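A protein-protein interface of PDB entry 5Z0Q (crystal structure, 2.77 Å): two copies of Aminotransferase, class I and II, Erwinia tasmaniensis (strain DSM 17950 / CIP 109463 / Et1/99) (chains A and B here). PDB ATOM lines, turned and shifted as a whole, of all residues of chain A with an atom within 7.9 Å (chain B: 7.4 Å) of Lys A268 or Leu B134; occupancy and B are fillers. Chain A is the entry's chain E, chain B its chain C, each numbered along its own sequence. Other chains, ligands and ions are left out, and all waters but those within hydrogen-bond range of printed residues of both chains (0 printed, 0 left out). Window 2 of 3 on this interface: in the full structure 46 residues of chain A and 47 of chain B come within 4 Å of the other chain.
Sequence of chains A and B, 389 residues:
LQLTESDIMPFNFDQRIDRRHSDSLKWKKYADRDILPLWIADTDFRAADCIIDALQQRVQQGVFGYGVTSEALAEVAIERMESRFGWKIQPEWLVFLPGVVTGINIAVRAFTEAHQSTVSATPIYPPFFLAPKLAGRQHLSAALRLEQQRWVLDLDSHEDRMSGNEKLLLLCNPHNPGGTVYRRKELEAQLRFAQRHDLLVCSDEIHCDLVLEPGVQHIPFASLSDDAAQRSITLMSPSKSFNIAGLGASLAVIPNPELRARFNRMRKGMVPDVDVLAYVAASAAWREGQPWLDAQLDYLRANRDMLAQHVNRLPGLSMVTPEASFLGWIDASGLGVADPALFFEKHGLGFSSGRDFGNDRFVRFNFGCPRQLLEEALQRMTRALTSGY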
ATOM      1  N   ILE A 106      33.095  -0.553  18.788  1.00  0.00           N
ATOM      2  CA  ILE A 106      32.395  -1.256  19.858  1.00  0.00           C
ATOM      3  C   ILE A 106      33.096  -1.026  21.191  1.00  0.00           C
ATOM      4  O   ILE A 106      32.447  -0.788  22.216  1.00  0.00           O
ATOM      5  CB  ILE A 106      32.270  -2.756  19.530  1.00  0.00           C
ATOM      6  CG1 ILE A 106      31.400  -2.966  18.289  1.00  0.00           C
ATOM      7  CG2 ILE A 106      31.673  -3.511  20.706  1.00  0.00           C
ATOM      8  CD1 ILE A 106      31.307  -4.410  17.847  1.00  0.00           C
ATOM      9  N   ARG A 262      29.893  -6.968  28.042  1.00  0.00           N
ATOM     10  CA  ARG A 262      29.618  -5.619  27.557  1.00  0.00           C
ATOM     11  C   ARG A 262      29.883  -5.509  26.062  1.00  0.00           C
ATOM     12  O   ARG A 262      29.110  -4.880  25.330  1.00  0.00           O
ATOM     13  CB  ARG A 262      30.464  -4.604  28.329  1.00  0.00           C
ATOM     14  CG  ARG A 262      29.691  -3.782  29.345  1.00  0.00           C
ATOM     15  CD  ARG A 262      29.034  -2.567  28.703  1.00  0.00           C
ATOM     16  NE  ARG A 262      28.196  -1.837  29.649  1.00  0.00           N
ATOM     17  CZ  ARG A 262      27.705  -0.620  29.431  1.00  0.00           C
ATOM     18  NH1 ARG A 262      27.974   0.013  28.298  1.00  0.00           N
ATOM     19  NH2 ARG A 262      26.948  -0.034  30.349  1.00  0.00           N
ATOM     20  N   PHE A 263      30.972  -6.121  25.592  1.00  0.00           N
ATOM     21  CA  PHE A 263      31.309  -6.068  24.173  1.00  0.00           C
ATOM     22  C   PHE A 263      30.242  -6.758  23.332  1.00  0.00           C
ATOM     23  O   PHE A 263      29.751  -6.196  22.345  1.00  0.00           O
ATOM     24  CB  PHE A 263      32.680  -6.709  23.946  1.00  0.00           C
ATOM     25  CG  PHE A 263      33.272  -6.432  22.591  1.00  0.00           C
ATOM     26  CD1 PHE A 263      32.944  -7.220  21.497  1.00  0.00           C
ATOM     27  CD2 PHE A 263      34.175  -5.395  22.417  1.00  0.00           C
ATOM     28  CE1 PHE A 263      33.495  -6.969  20.252  1.00  0.00           C
ATOM     29  CE2 PHE A 263      34.730  -5.140  21.175  1.00  0.00           C
ATOM     30  CZ  PHE A 263      34.389  -5.927  20.091  1.00  0.00           C
ATOM     31  N   ASN A 264      29.864  -7.980  23.716  1.00  0.00           N
ATOM     32  CA  ASN A 264      28.871  -8.724  22.946  1.00  0.00           C
ATOM     33  C   ASN A 264      27.505  -8.053  23.006  1.00  0.00           C
ATOM     34  O   ASN A 264      26.771  -8.040  22.010  1.00  0.00           O
ATOM     35  CB  ASN A 264      28.789 -10.164  23.452  1.00  0.00           C
ATOM     36  CG  ASN A 264      30.063 -10.945  23.191  1.00  0.00           C
ATOM     37  OD1 ASN A 264      30.765 -10.700  22.210  1.00  0.00           O
ATOM     38  ND2 ASN A 264      30.368 -11.891  24.072  1.00  0.00           N
ATOM     39  N   ARG A 265      27.145  -7.490  24.161  1.00  0.00           N
ATOM     40  CA  ARG A 265      25.883  -6.766  24.268  1.00  0.00           C
ATOM     41  C   ARG A 265      25.883  -5.538  23.367  1.00  0.00           C
ATOM     42  O   ARG A 265      24.866  -5.210  22.746  1.00  0.00           O
ATOM     43  CB  ARG A 265      25.628  -6.373  25.724  1.00  0.00           C
ATOM     44  CG  ARG A 265      24.160  -6.194  26.102  1.00  0.00           C
ATOM     45  CD  ARG A 265      23.629  -4.817  25.732  1.00  0.00           C
ATOM     46  NE  ARG A 265      22.260  -4.617  26.200  1.00  0.00           N
ATOM     47  CZ  ARG A 265      21.546  -3.518  25.983  1.00  0.00           C
ATOM     48  NH1 ARG A 265      22.067  -2.509  25.298  1.00  0.00           N
ATOM     49  NH2 ARG A 265      20.307  -3.425  26.449  1.00  0.00           N
ATOM     50  N   MET A 266      27.024  -4.853  23.273  1.00  0.00           N
ATOM     51  CA  MET A 266      27.136  -3.673  22.427  1.00  0.00           C
ATOM     52  C   MET A 266      27.190  -4.012  20.943  1.00  0.00           C
ATOM     53  O   MET A 266      27.052  -3.106  20.114  1.00  0.00           O
ATOM     54  CB  MET A 266      28.377  -2.869  22.824  1.00  0.00           C
ATOM     55  CG  MET A 266      28.202  -1.362  22.735  1.00  0.00           C
ATOM     56  SD  MET A 266      26.895  -0.773  23.828  1.00  0.00           S
ATOM     57  CE  MET A 266      27.415  -1.477  25.391  1.00  0.00           C
ATOM     58  N   ARG A 267      27.381  -5.284  20.590  1.00  0.00           N
ATOM     59  CA  ARG A 267      27.460  -5.714  19.201  1.00  0.00           C
ATOM     60  C   ARG A 267      26.135  -6.227  18.649  1.00  0.00           C
ATOM     61  O   ARG A 267      25.846  -6.005  17.469  1.00  0.00           O
ATOM     62  CB  ARG A 267      28.516  -6.814  19.045  1.00  0.00           C
ATOM     63  CG  ARG A 267      28.532  -7.439  17.666  1.00  0.00           C
ATOM     64  CD  ARG A 267      29.379  -8.686  17.591  1.00  0.00           C
ATOM     65  NE  ARG A 267      29.362  -9.240  16.243  1.00  0.00           N
ATOM     66  CZ  ARG A 267      30.047 -10.316  15.870  1.00  0.00           C
ATOM     67  NH1 ARG A 267      29.974 -10.749  14.620  1.00  0.00           N
ATOM     68  NH2 ARG A 267      30.805 -10.958  16.750  1.00  0.00           N
ATOM     69  N   LYS A 268      25.325  -6.884  19.478  1.00  0.00           N
ATOM     70  CA  LYS A 268      24.122  -7.572  19.020  1.00  0.00           C
ATOM     71  C   LYS A 268      23.232  -6.660  18.186  1.00  0.00           C
ATOM     72  O   LYS A 268      22.999  -5.504  18.546  1.00  0.00           O
ATOM     73  CB  LYS A 268      23.346  -8.109  20.223  1.00  0.00           C
ATOM     74  CG  LYS A 268      23.322  -9.622  20.328  1.00  0.00           C
ATOM     75  CD  LYS A 268      22.511 -10.246  19.203  1.00  0.00           C
ATOM     76  CE  LYS A 268      22.450 -11.758  19.350  1.00  0.00           C
ATOM     77  NZ  LYS A 268      21.602 -12.391  18.302  1.00  0.00           N
ATOM     78  N   GLY A 269      22.734  -7.192  17.079  1.00  0.00           N
ATOM     79  CA  GLY A 269      21.882  -6.435  16.148  1.00  0.00           C
ATOM     80  C   GLY A 269      22.582  -5.421  15.263  1.00  0.00           C
ATOM     81  O   GLY A 269      22.339  -5.370  14.058  1.00  0.00           O
ATOM     82  N   MET A 270      23.468  -4.616  15.850  1.00  0.00           N
ATOM     83  CA  MET A 270      24.144  -3.568  15.092  1.00  0.00           C
ATOM     84  C   MET A 270      25.173  -4.157  14.133  1.00  0.00           C
ATOM     85  O   MET A 270      25.189  -3.824  12.944  1.00  0.00           O
ATOM     86  CB  MET A 270      24.803  -2.580  16.054  1.00  0.00           C
ATOM     87  CG  MET A 270      24.965  -1.185  15.490  1.00  0.00           C
ATOM     88  SD  MET A 270      23.393  -0.325  15.296  1.00  0.00           S
ATOM     89  CE  MET A 270      23.972   1.319  14.884  1.00  0.00           C
ATOM     90  N   VAL A 271      26.026  -5.040  14.630  1.00  0.00           N
ATOM     91  CA  VAL A 271      27.107  -5.632  13.845  1.00  0.00           C
ATOM     92  C   VAL A 271      26.722  -7.067  13.499  1.00  0.00           C
ATOM     93  O   VAL A 271      26.390  -7.840  14.408  1.00  0.00           O
ATOM     94  CB  VAL A 271      28.442  -5.594  14.611  1.00  0.00           C
ATOM     95  CG1 VAL A 271      29.556  -6.178  13.765  1.00  0.00           C
ATOM     96  CG2 VAL A 271      28.773  -4.171  15.033  1.00  0.00           C
ATOM     97  N   PRO A 272      26.757  -7.456  12.231  1.00  0.00           N
ATOM     98  CA  PRO A 272      26.324  -8.799  11.838  1.00  0.00           C
ATOM     99  C   PRO A 272      27.429  -9.827  12.063  1.00  0.00           C
ATOM    100  O   PRO A 272      28.532  -9.513  12.509  1.00  0.00           O
ATOM    101  CB  PRO A 272      26.013  -8.632  10.352  1.00  0.00           C
ATOM    102  CG  PRO A 272      26.988  -7.595   9.906  1.00  0.00           C
ATOM    103  CD  PRO A 272      27.151  -6.642  11.067  1.00  0.00           C
ATOM    104  N   ASP A 273      27.108 -11.076  11.736  1.00  0.00           N
ATOM    105  CA  ASP A 273      28.082 -12.151  11.813  1.00  0.00           C
ATOM    106  C   ASP A 273      29.109 -12.022  10.692  1.00  0.00           C
ATOM    107  O   ASP A 273      28.917 -11.291   9.715  1.00  0.00           O
ATOM    108  CB  ASP A 273      27.386 -13.510  11.728  1.00  0.00           C
ATOM    109  CG  ASP A 273      26.409 -13.739  12.866  1.00  0.00           C
ATOM    110  OD1 ASP A 273      26.792 -13.519  14.034  1.00  0.00           O
ATOM    111  OD2 ASP A 273      25.255 -14.135  12.591  1.00  0.00           O
ATOM    112  N   VAL B 101      19.076  -7.338   9.323  1.00  0.00           N
ATOM    113  CA  VAL B 101      18.906  -7.145  10.761  1.00  0.00           C
ATOM    114  C   VAL B 101      19.620  -5.880  11.217  1.00  0.00           C
ATOM    115  O   VAL B 101      19.115  -5.136  12.068  1.00  0.00           O
ATOM    116  CB  VAL B 101      19.403  -8.385  11.530  1.00  0.00           C
ATOM    117  CG1 VAL B 101      19.272  -8.170  13.033  1.00  0.00           C
ATOM    118  CG2 VAL B 101      18.628  -9.617  11.097  1.00  0.00           C
ATOM    119  N   ASN B 105      18.146  -2.389  13.209  1.00  0.00           N
ATOM    120  CA  ASN B 105      18.699  -1.803  14.425  1.00  0.00           C
ATOM    121  C   ASN B 105      19.085  -0.344  14.211  1.00  0.00           C
ATOM    122  O   ASN B 105      18.753   0.519  15.031  1.00  0.00           O
ATOM    123  CB  ASN B 105      19.898  -2.620  14.903  1.00  0.00           C
ATOM    124  CG  ASN B 105      19.484  -3.906  15.593  1.00  0.00           C
ATOM    125  OD1 ASN B 105      19.457  -3.984  16.821  1.00  0.00           O
ATOM    126  ND2 ASN B 105      19.153  -4.921  14.804  1.00  0.00           N
ATOM    127  N   VAL B 108      16.117   1.989  14.298  1.00  0.00           N
ATOM    128  CA  VAL B 108      15.568   2.259  15.623  1.00  0.00           C
ATOM    129  C   VAL B 108      16.472   3.213  16.397  1.00  0.00           C
ATOM    130  O   VAL B 108      15.994   4.122  17.086  1.00  0.00           O
ATOM    131  CB  VAL B 108      15.343   0.940  16.384  1.00  0.00           C
ATOM    132  CG1 VAL B 108      14.860   1.213  17.800  1.00  0.00           C
ATOM    133  CG2 VAL B 108      14.344   0.066  15.642  1.00  0.00           C
ATOM    134  N   ARG B 109      17.792   3.030  16.292  1.00  0.00           N
ATOM    135  CA  ARG B 109      18.716   3.895  17.020  1.00  0.00           C
ATOM    136  C   ARG B 109      18.735   5.309  16.451  1.00  0.00           C
ATOM    137  O   ARG B 109      19.025   6.262  17.182  1.00  0.00           O
ATOM    138  CB  ARG B 109      20.128   3.307  16.994  1.00  0.00           C
ATOM    139  CG  ARG B 109      20.223   1.842  17.386  1.00  0.00           C
ATOM    140  CD  ARG B 109      20.582   1.653  18.847  1.00  0.00           C
ATOM    141  NE  ARG B 109      20.625   0.236  19.201  1.00  0.00           N
ATOM    142  CZ  ARG B 109      21.706  -0.532  19.093  1.00  0.00           C
ATOM    143  NH1 ARG B 109      22.846  -0.023  18.646  1.00  0.00           N
ATOM    144  NH2 ARG B 109      21.648  -1.811  19.438  1.00  0.00           N
ATOM    145  N   PHE B 129      11.049  -6.506  17.685  1.00  0.00           N
ATOM    146  CA  PHE B 129      10.923  -6.042  19.060  1.00  0.00           C
ATOM    147  C   PHE B 129      12.188  -6.265  19.876  1.00  0.00           C
ATOM    148  O   PHE B 129      12.265  -5.789  21.014  1.00  0.00           O
ATOM    149  CB  PHE B 129       9.727  -6.714  19.752  1.00  0.00           C
ATOM    150  CG  PHE B 129       9.756  -8.214  19.710  1.00  0.00           C
ATOM    151  CD1 PHE B 129       9.175  -8.902  18.657  1.00  0.00           C
ATOM    152  CD2 PHE B 129      10.345  -8.938  20.733  1.00  0.00           C
ATOM    153  CE1 PHE B 129       9.193 -10.282  18.618  1.00  0.00           C
ATOM    154  CE2 PHE B 129      10.366 -10.320  20.700  1.00  0.00           C
ATOM    155  CZ  PHE B 129       9.789 -10.992  19.641  1.00  0.00           C
ATOM    156  N   LEU B 130      13.179  -6.968  19.322  1.00  0.00           N
ATOM    157  CA  LEU B 130      14.470  -7.092  19.988  1.00  0.00           C
ATOM    158  C   LEU B 130      15.321  -5.842  19.813  1.00  0.00           C
ATOM    159  O   LEU B 130      16.106  -5.503  20.705  1.00  0.00           O
ATOM    160  CB  LEU B 130      15.224  -8.314  19.459  1.00  0.00           C
ATOM    161  CG  LEU B 130      15.317  -9.522  20.395  1.00  0.00           C
ATOM    162  CD1 LEU B 130      13.932 -10.015  20.790  1.00  0.00           C
ATOM    163  CD2 LEU B 130      16.124 -10.639  19.749  1.00  0.00           C
ATOM    164  N   ALA B 131      15.182  -5.148  18.678  1.00  0.00           N
ATOM    165  CA  ALA B 131      15.960  -3.928  18.469  1.00  0.00           C
ATOM    166  C   ALA B 131      15.563  -2.818  19.437  1.00  0.00           C
ATOM    167  O   ALA B 131      16.463  -2.197  20.028  1.00  0.00           O
ATOM    168  CB  ALA B 131      15.855  -3.483  17.007  1.00  0.00           C
ATOM    169  N   PRO B 132      14.276  -2.507  19.649  1.00  0.00           N
ATOM    170  CA  PRO B 132      13.946  -1.526  20.697  1.00  0.00           C
ATOM    171  C   PRO B 132      14.354  -1.987  22.083  1.00  0.00           C
ATOM    172  O   PRO B 132      14.641  -1.153  22.950  1.00  0.00           O
ATOM    173  CB  PRO B 132      12.421  -1.381  20.578  1.00  0.00           C
ATOM    174  CG  PRO B 132      12.097  -1.844  19.205  1.00  0.00           C
ATOM    175  CD  PRO B 132      13.070  -2.939  18.922  1.00  0.00           C
ATOM    176  N   LYS B 133      14.391  -3.301  22.311  1.00  0.00           N
ATOM    177  CA  LYS B 133      14.815  -3.823  23.604  1.00  0.00           C
ATOM    178  C   LYS B 133      16.287  -3.521  23.863  1.00  0.00           C
ATOM    179  O   LYS B 133      16.658  -3.120  24.972  1.00  0.00           O
ATOM    180  CB  LYS B 133      14.547  -5.326  23.660  1.00  0.00           C
ATOM    181  CG  LYS B 133      14.735  -5.965  25.023  1.00  0.00           C
ATOM    182  CD  LYS B 133      14.387  -7.445  24.960  1.00  0.00           C
ATOM    183  CE  LYS B 133      14.553  -8.120  26.309  1.00  0.00           C
ATOM    184  NZ  LYS B 133      14.212  -9.567  26.231  1.00  0.00           N
ATOM    185  N   LEU B 134      17.137  -3.698  22.850  1.00  0.00           N
ATOM    186  CA  LEU B 134      18.559  -3.421  23.000  1.00  0.00           C
ATOM    187  C   LEU B 134      18.879  -1.935  22.934  1.00  0.00           C
ATOM    188  O   LEU B 134      19.947  -1.524  23.400  1.00  0.00           O
ATOM    189  CB  LEU B 134      19.358  -4.160  21.925  1.00  0.00           C
ATOM    190  CG  LEU B 134      19.155  -5.673  21.840  1.00  0.00           C
ATOM    191  CD1 LEU B 134      20.060  -6.275  20.775  1.00  0.00           C
ATOM    192  CD2 LEU B 134      19.394  -6.328  23.192  1.00  0.00           C
ATOM    193  N   ALA B 135      17.987  -1.126  22.368  1.00  0.00           N
ATOM    194  CA  ALA B 135      18.196   0.310  22.252  1.00  0.00           C
ATOM    195  C   ALA B 135      17.536   1.099  23.375  1.00  0.00           C
ATOM    196  O   ALA B 135      17.577   2.333  23.353  1.00  0.00           O
ATOM    197  CB  ALA B 135      17.678   0.810  20.899  1.00  0.00           C
ATOM    198  N   GLY B 136      16.935   0.423  24.351  1.00  0.00           N
ATOM    199  CA  GLY B 136      16.268   1.119  25.434  1.00  0.00           C
ATOM    200  C   GLY B 136      14.960   1.770  25.045  1.00  0.00           C
ATOM    201  O   GLY B 136      14.593   2.800  25.618  1.00  0.00           O
ATOM    202  N   ARG B 137      14.244   1.194  24.084  1.00  0.00           N
ATOM    203  CA  ARG B 137      12.976   1.729  23.607  1.00  0.00           C
ATOM    204  C   ARG B 137      11.854   0.760  23.953  1.00  0.00           C
ATOM    205  O   ARG B 137      11.967  -0.443  23.694  1.00  0.00           O
ATOM    206  CB  ARG B 137      13.012   1.961  22.095  1.00  0.00           C
ATOM    207  CG  ARG B 137      14.229   2.718  21.595  1.00  0.00           C
ATOM    208  CD  ARG B 137      14.310   4.105  22.202  1.00  0.00           C
ATOM    209  NE  ARG B 137      15.081   5.018  21.362  1.00  0.00           N
ATOM    210  CZ  ARG B 137      16.405   5.136  21.401  1.00  0.00           C
ATOM    211  NH1 ARG B 137      17.117   4.396  22.240  1.00  0.00           N
ATOM    212  NH2 ARG B 137      17.018   5.994  20.598  1.00  0.00           N
ATOM    213  N   MET B 270      30.305   1.908  13.062  1.00  0.00           N
ATOM    214  CA  MET B 270      29.758   0.800  13.833  1.00  0.00           C
ATOM    215  C   MET B 270      29.410  -0.391  12.945  1.00  0.00           C
ATOM    216  O   MET B 270      29.594  -1.544  13.350  1.00  0.00           O
ATOM    217  CB  MET B 270      28.527   1.270  14.607  1.00  0.00           C
ATOM    218  CG  MET B 270      28.119   0.354  15.741  1.00  0.00           C
ATOM    219  SD  MET B 270      29.351   0.267  17.053  1.00  0.00           S
ATOM    220  CE  MET B 270      28.502  -0.779  18.234  1.00  0.00           C
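CG1 of Ile A106 touches CE of Met B270, at 3.6 Å. Lys B133 touches Arg A265. Met A266 touches Met B270 (O to CE, 3.3 Å). Lys A268 touches Leu B134. O of Gly A269 touches O of Val B101 (3.8 Å). Met A270 touches Met B270 (CG to CG, 3.5 Å). CG2 of Val A271 touches O of Met B270 (3.2 Å).
Met A270 touches its own counterpart, Met B270. 1 position is printed for both chains. Of the 10 pairs that touch across the chains among the printed residues, 1 has its exchanged pair printed and touching as well.
Of the 14 printed residues of chain B, 6 touch a printed residue of chain A. Hydrophobic or aromatic side chains of chain B that line the printed part of chain A: Leu B134 and Met B270. Of the 13 printed residues of chain A, 7 touch a printed residue of chain B. Among the printed residues, no Asp or Glu carboxylate lies within 4 Å of a Lys or Arg side-chain nitrogen of the other chain.
O of Val B101 sits at hydrogen-bond distance from ND2 of Asn B105, 2.7 Å away.
Of the printed residues of chain B, Lys A268 touches Leu B134 (3.8 Å). Leu B134 touches two residues of chain A. Printed residues of chain B within 4 Å of Val A271: Met B270 (3.2 Å). Of the printed residues of chain A, Lys B133 touches Arg A265. Of the printed residues of chain A, Arg B109 touches Met A270 (3.4 Å). Printed residues of chain B within 4 Å of Met A270: Arg B109 (3.4 Å) and Met B270 (3.5 Å). Phe B129 touches none of the printed residues of chain A. Arg A267 touches none of the printed residues of chain B.
The backbone carbonyl oxygen (O) of Gly A269 is in hydrogen-bond range of the side-chain amide nitrogen (ND2) of Asn B105. The side-chain sulfur (SD) of Met A270 lies within hydrogen-bond range of the guanidinium group (NH1) of Arg B109 (3.4 Å). The backbone carbonyl oxygen of Leu B134 sits at hydrogen-bond distance from the guanidinium group of Arg A265, 3.0 Å away.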
